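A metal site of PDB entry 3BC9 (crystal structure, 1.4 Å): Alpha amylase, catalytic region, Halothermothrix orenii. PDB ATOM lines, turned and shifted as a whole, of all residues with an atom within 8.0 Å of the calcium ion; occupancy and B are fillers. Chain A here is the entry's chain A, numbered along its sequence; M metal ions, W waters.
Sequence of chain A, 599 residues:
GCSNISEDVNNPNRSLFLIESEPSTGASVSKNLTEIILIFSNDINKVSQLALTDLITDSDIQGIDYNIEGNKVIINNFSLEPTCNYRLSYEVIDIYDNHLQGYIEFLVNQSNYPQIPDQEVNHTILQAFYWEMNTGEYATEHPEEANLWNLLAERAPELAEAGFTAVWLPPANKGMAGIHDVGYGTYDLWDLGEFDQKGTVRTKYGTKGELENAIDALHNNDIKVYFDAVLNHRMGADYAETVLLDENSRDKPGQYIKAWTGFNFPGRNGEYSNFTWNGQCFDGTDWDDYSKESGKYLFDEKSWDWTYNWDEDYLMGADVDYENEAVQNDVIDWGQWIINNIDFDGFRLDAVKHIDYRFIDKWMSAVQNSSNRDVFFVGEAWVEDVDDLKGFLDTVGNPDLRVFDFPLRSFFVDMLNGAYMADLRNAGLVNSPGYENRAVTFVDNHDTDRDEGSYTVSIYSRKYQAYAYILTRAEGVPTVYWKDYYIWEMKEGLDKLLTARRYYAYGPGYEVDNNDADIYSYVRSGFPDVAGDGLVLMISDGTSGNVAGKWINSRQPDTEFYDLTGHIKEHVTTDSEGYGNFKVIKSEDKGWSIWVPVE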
ATOM      1  N   PRO A 114      -2.688  17.516 -17.175  1.00  0.00           N
ATOM      2  CA  PRO A 114      -1.367  17.254 -17.797  1.00  0.00           C
ATOM      3  C   PRO A 114      -1.198  15.766 -17.998  1.00  0.00           C
ATOM      4  O   PRO A 114      -1.686  14.978 -17.205  1.00  0.00           O
ATOM      5  CB  PRO A 114      -0.394  17.774 -16.746  1.00  0.00           C
ATOM      6  CG  PRO A 114      -1.184  18.791 -16.010  1.00  0.00           C
ATOM      7  CD  PRO A 114      -2.595  18.340 -15.940  1.00  0.00           C
ATOM      8  N   ILE A 116       1.083  12.894 -17.877  1.00  0.00           N
ATOM      9  CA  ILE A 116       2.310  12.485 -17.258  1.00  0.00           C
ATOM     10  C   ILE A 116       2.598  11.072 -17.760  1.00  0.00           C
ATOM     11  O   ILE A 116       1.764  10.193 -17.651  1.00  0.00           O
ATOM     12  CB  ILE A 116       2.170  12.448 -15.716  1.00  0.00           C
ATOM     13  CG1 ILE A 116       1.640  13.813 -15.151  1.00  0.00           C
ATOM     14  CG2 ILE A 116       3.500  12.017 -15.159  1.00  0.00           C
ATOM     15  CD1 ILE A 116       2.476  14.976 -15.476  1.00  0.00           C
ATOM     16  N   TYR A 504       0.246  17.425 -11.080  1.00  0.00           N
ATOM     17  CA  TYR A 504       0.971  18.653 -11.067  1.00  0.00           C
ATOM     18  C   TYR A 504       2.312  18.690 -10.390  1.00  0.00           C
ATOM     19  O   TYR A 504       3.143  19.543 -10.773  1.00  0.00           O
ATOM     20  CB  TYR A 504       0.114  19.793 -10.533  1.00  0.00           C
ATOM     21  CG  TYR A 504      -1.192  20.001 -11.283  1.00  0.00           C
ATOM     22  CD1 TYR A 504      -2.375  19.381 -10.872  1.00  0.00           C
ATOM     23  CD2 TYR A 504      -1.202  20.751 -12.492  1.00  0.00           C
ATOM     24  CE1 TYR A 504      -3.574  19.589 -11.595  1.00  0.00           C
ATOM     25  CE2 TYR A 504      -2.339  20.966 -13.176  1.00  0.00           C
ATOM     26  CZ  TYR A 504      -3.508  20.377 -12.762  1.00  0.00           C
ATOM     27  OH  TYR A 504      -4.775  20.535 -13.429  1.00  0.00           O
ATOM     28  N   TYR A 506       5.420  17.828 -10.204  1.00  0.00           N
ATOM     29  CA  TYR A 506       6.456  17.240 -11.085  1.00  0.00           C
ATOM     30  C   TYR A 506       7.561  18.255 -11.392  1.00  0.00           C
ATOM     31  O   TYR A 506       7.414  19.497 -11.330  1.00  0.00           O
ATOM     32  CB  TYR A 506       5.882  16.711 -12.412  1.00  0.00           C
ATOM     33  CG  TYR A 506       4.964  15.575 -12.192  1.00  0.00           C
ATOM     34  CD1 TYR A 506       3.599  15.753 -12.069  1.00  0.00           C
ATOM     35  CD2 TYR A 506       5.462  14.326 -11.954  1.00  0.00           C
ATOM     36  CE1 TYR A 506       2.761  14.691 -11.725  1.00  0.00           C
ATOM     37  CE2 TYR A 506       4.638  13.283 -11.601  1.00  0.00           C
ATOM     38  CZ  TYR A 506       3.319  13.453 -11.548  1.00  0.00           C
ATOM     39  OH  TYR A 506       2.488  12.379 -11.177  1.00  0.00           O
ATOM     40  N   GLY A 507       8.687  17.674 -11.787  1.00  0.00           N
ATOM     41  CA  GLY A 507       9.841  18.525 -12.132  1.00  0.00           C
ATOM     42  C   GLY A 507      10.600  18.894 -10.876  1.00  0.00           C
ATOM     43  O   GLY A 507      10.264  18.518  -9.759  1.00  0.00           O
ATOM     44  N   ARG A 524       7.061  23.708  -7.626  1.00  0.00           N
ATOM     45  CA  ARG A 524       7.459  22.616  -8.533  1.00  0.00           C
ATOM     46  C   ARG A 524       7.331  23.174  -9.927  1.00  0.00           C
ATOM     47  O   ARG A 524       6.263  23.691 -10.280  1.00  0.00           O
ATOM     48  CB  ARG A 524       6.553  21.415  -8.443  1.00  0.00           C
ATOM     49  CG  ARG A 524       6.524  20.789  -7.059  1.00  0.00           C
ATOM     50  CD  ARG A 524       7.848  20.132  -6.650  1.00  0.00           C
ATOM     51  NE  ARG A 524       8.318  19.085  -7.572  1.00  0.00           N
ATOM     52  CZ  ARG A 524       7.898  17.815  -7.514  1.00  0.00           C
ATOM     53  NH1 ARG A 524       7.016  17.399  -6.623  1.00  0.00           N
ATOM     54  NH2 ARG A 524       8.341  16.925  -8.343  1.00  0.00           N
ATOM     55  N   SER A 525       8.411  23.149 -10.715  1.00  0.00           N
ATOM     56  CA  SER A 525       8.387  23.811 -12.005  1.00  0.00           C
ATOM     57  C   SER A 525       7.665  23.035 -13.092  1.00  0.00           C
ATOM     58  O   SER A 525       7.313  23.656 -14.111  1.00  0.00           O
ATOM     59  CB  SER A 525       9.784  24.126 -12.498  1.00  0.00           C
ATOM     60  OG  SER A 525      10.466  22.926 -12.669  1.00  0.00           O
ATOM     61  N   GLY A 526       7.352  21.767 -12.879  1.00  0.00           N
ATOM     62  CA  GLY A 526       6.842  20.925 -13.941  1.00  0.00           C
ATOM     63  C   GLY A 526       7.971  20.389 -14.802  1.00  0.00           C
ATOM     64  O   GLY A 526       9.083  20.859 -14.711  1.00  0.00           O
ATOM     65  N   PHE A 527       7.666  19.429 -15.623  1.00  0.00           N
ATOM     66  CA  PHE A 527       8.604  18.920 -16.617  1.00  0.00           C
ATOM     67  C   PHE A 527       8.607  19.841 -17.820  1.00  0.00           C
ATOM     68  O   PHE A 527       7.540  20.315 -18.257  1.00  0.00           O
ATOM     69  CB  PHE A 527       8.139  17.542 -17.062  1.00  0.00           C
ATOM     70  CG  PHE A 527       8.288  16.447 -16.034  1.00  0.00           C
ATOM     71  CD1 PHE A 527       7.248  15.556 -15.811  1.00  0.00           C
ATOM     72  CD2 PHE A 527       9.499  16.204 -15.409  1.00  0.00           C
ATOM     73  CE1 PHE A 527       7.366  14.498 -14.912  1.00  0.00           C
ATOM     74  CE2 PHE A 527       9.624  15.148 -14.490  1.00  0.00           C
ATOM     75  CZ  PHE A 527       8.562  14.279 -14.269  1.00  0.00           C
ATOM     76  N   PRO A 528       9.789  20.076 -18.392  1.00  0.00           N
ATOM     77  CA  PRO A 528       9.895  20.990 -19.532  1.00  0.00           C
ATOM     78  C   PRO A 528       9.127  20.470 -20.764  1.00  0.00           C
ATOM     79  O   PRO A 528       8.602  21.259 -21.513  1.00  0.00           O
ATOM     80  CB  PRO A 528      11.401  21.058 -19.786  1.00  0.00           C
ATOM     81  CG  PRO A 528      11.932  19.800 -19.230  1.00  0.00           C
ATOM     82  CD  PRO A 528      11.087  19.505 -18.020  1.00  0.00           C
ATOM     83  N   ASP A 529       8.953  19.159 -20.852  1.00  0.00           N
ATOM     84  CA  ASP A 529       8.272  18.521 -21.990  1.00  0.00           C
ATOM     85  C   ASP A 529       6.815  18.082 -21.736  1.00  0.00           C
ATOM     86  O   ASP A 529       6.214  17.355 -22.541  1.00  0.00           O
ATOM     87  CB  ASP A 529       9.106  17.338 -22.485  1.00  0.00           C
ATOM     88  CG  ASP A 529       9.504  16.364 -21.370  1.00  0.00           C
ATOM     89  OD1 ASP A 529       9.238  16.589 -20.158  1.00  0.00           O
ATOM     90  OD2 ASP A 529      10.137  15.327 -21.703  1.00  0.00           O
ATOM     91  N   VAL A 530       6.225  18.518 -20.615  1.00  0.00           N
ATOM     92  CA  VAL A 530       4.836  18.214 -20.292  1.00  0.00           C
ATOM     93  C   VAL A 530       4.129  19.539 -20.190  1.00  0.00           C
ATOM     94  O   VAL A 530       4.573  20.446 -19.464  1.00  0.00           O
ATOM     95  CB  VAL A 530       4.686  17.417 -18.955  1.00  0.00           C
ATOM     96  CG1 VAL A 530       3.193  17.371 -18.507  1.00  0.00           C
ATOM     97  CG2 VAL A 530       5.281  16.017 -19.079  1.00  0.00           C
ATOM     98  N   ALA A 531       3.051  19.709 -20.956  1.00  0.00           N
ATOM     99  CA  ALA A 531       2.247  20.909 -20.868  1.00  0.00           C
ATOM    100  C   ALA A 531       1.375  20.907 -19.606  1.00  0.00           C
ATOM    101  O   ALA A 531       0.625  19.971 -19.354  1.00  0.00           O
ATOM    102  CB  ALA A 531       1.354  21.094 -22.118  1.00  0.00           C
ATOM    103  N   GLY A 532       1.417  22.005 -18.862  1.00  0.00           N
ATOM    104  CA  GLY A 532       0.372  22.291 -17.895  1.00  0.00           C
ATOM    105  C   GLY A 532       0.630  21.817 -16.472  1.00  0.00           C
ATOM    106  O   GLY A 532      -0.256  21.987 -15.653  1.00  0.00           O
ATOM    107  N   ASP A 533       1.756  21.161 -16.205  1.00  0.00           N
ATOM    108  CA  ASP A 533       2.084  20.695 -14.865  1.00  0.00           C
ATOM    109  C   ASP A 533       2.835  21.777 -14.100  1.00  0.00           C
ATOM    110  O   ASP A 533       2.983  22.905 -14.547  1.00  0.00           O
ATOM    111  CB  ASP A 533       2.862  19.376 -14.894  1.00  0.00           C
ATOM    112  CG  ASP A 533       4.193  19.482 -15.572  1.00  0.00           C
ATOM    113  OD1 ASP A 533       4.545  20.500 -16.255  1.00  0.00           O
ATOM    114  OD2 ASP A 533       4.994  18.527 -15.379  1.00  0.00           O
ATOM    115  N   GLY A 534       3.238  21.459 -12.877  1.00  0.00           N
ATOM    116  CA  GLY A 534       3.848  22.422 -11.973  1.00  0.00           C
ATOM    117  C   GLY A 534       2.859  23.014 -11.023  1.00  0.00           C
ATOM    118  O   GLY A 534       1.677  22.936 -11.246  1.00  0.00           O
ATOM    119  N   ARG A 555       8.548  29.783 -11.993  1.00  0.00           N
ATOM    120  CA  ARG A 555       9.334  29.198 -13.069  1.00  0.00           C
ATOM    121  C   ARG A 555       8.553  28.974 -14.364  1.00  0.00           C
ATOM    122  O   ARG A 555       9.040  28.313 -15.282  1.00  0.00           O
ATOM    123  CB  ARG A 555      10.097  27.937 -12.661  1.00  0.00           C
ATOM    124  CG  ARG A 555      11.475  28.172 -12.055  1.00  0.00           C
ATOM    125  CD  ARG A 555      11.380  28.582 -10.704  1.00  0.00           C
ATOM    126  NE  ARG A 555      12.674  28.779 -10.090  1.00  0.00           N
ATOM    127  CZ  ARG A 555      12.826  29.173  -8.825  1.00  0.00           C
ATOM    128  NH1 ARG A 555      11.741  29.400  -8.069  1.00  0.00           N
ATOM    129  NH2 ARG A 555      14.058  29.320  -8.347  1.00  0.00           N
ATOM    130  N   GLN A 556       7.383  29.597 -14.446  1.00  0.00           N
ATOM    131  CA  GLN A 556       6.510  29.517 -15.594  1.00  0.00           C
ATOM    132  C   GLN A 556       6.112  30.939 -16.012  1.00  0.00           C
ATOM    133  O   GLN A 556       5.135  31.507 -15.508  1.00  0.00           O
ATOM    134  CB  GLN A 556       5.271  28.670 -15.285  1.00  0.00           C
ATOM    135  CG  GLN A 556       5.627  27.263 -14.819  1.00  0.00           C
ATOM    136  CD  GLN A 556       4.544  26.302 -15.029  1.00  0.00           C
ATOM    137  OE1 GLN A 556       4.083  26.125 -16.172  1.00  0.00           O
ATOM    138  NE2 GLN A 556       4.097  25.655 -13.958  1.00  0.00           N
ATOM    139  N   PRO A 597      -1.418  25.553 -13.078  1.00  0.00           N
ATOM    140  CA  PRO A 597      -1.881  26.179 -14.309  1.00  0.00           C
ATOM    141  C   PRO A 597      -3.290  25.901 -14.710  1.00  0.00           C
ATOM    142  O   PRO A 597      -3.761  24.828 -14.539  1.00  0.00           O
ATOM    143  CB  PRO A 597      -0.873  25.720 -15.358  1.00  0.00           C
ATOM    144  CG  PRO A 597       0.329  25.218 -14.549  1.00  0.00           C
ATOM    145  CD  PRO A 597      -0.244  24.686 -13.276  1.00  0.00           C
HETATM  146 CA    CA M   1       5.575  21.655 -17.868  1.00  0.00          CA
HETATM  147  O   HOH W   1       3.889  23.429 -17.112  1.00  0.00           O
HETATM  148  O   HOH W   2       6.955  23.122 -16.748  1.00  0.00           O
HETATM  149  O   HOH W   3       6.064  23.080 -19.648  1.00  0.00           O
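The backbone carbonyl oxygen (O) of Asp 533 is in hydrogen-bond range of the side-chain amide nitrogen (NE2) of Gln 556.
Of the 19 residues printed, 3 come within 4 Å of the calcium ion.
The calcium ion is bound by the side-chain carboxylate of Asp 533 (2.2 Å), the backbone carbonyl oxygen of Val 530 (2.2 Å), water W2 (2.3 Å), water W3 (2.3 Å), the backbone carbonyl oxygen of Phe 527 (2.4 Å) and water W1 (2.6 Å). The calcium ion has six donor atoms within binding distance.
Water W1 lies within hydrogen-bond range of the backbone carbonyl oxygen of Asp 533, the side-chain amide oxygen of Gln 556 and the backbone NH of Gly 532.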
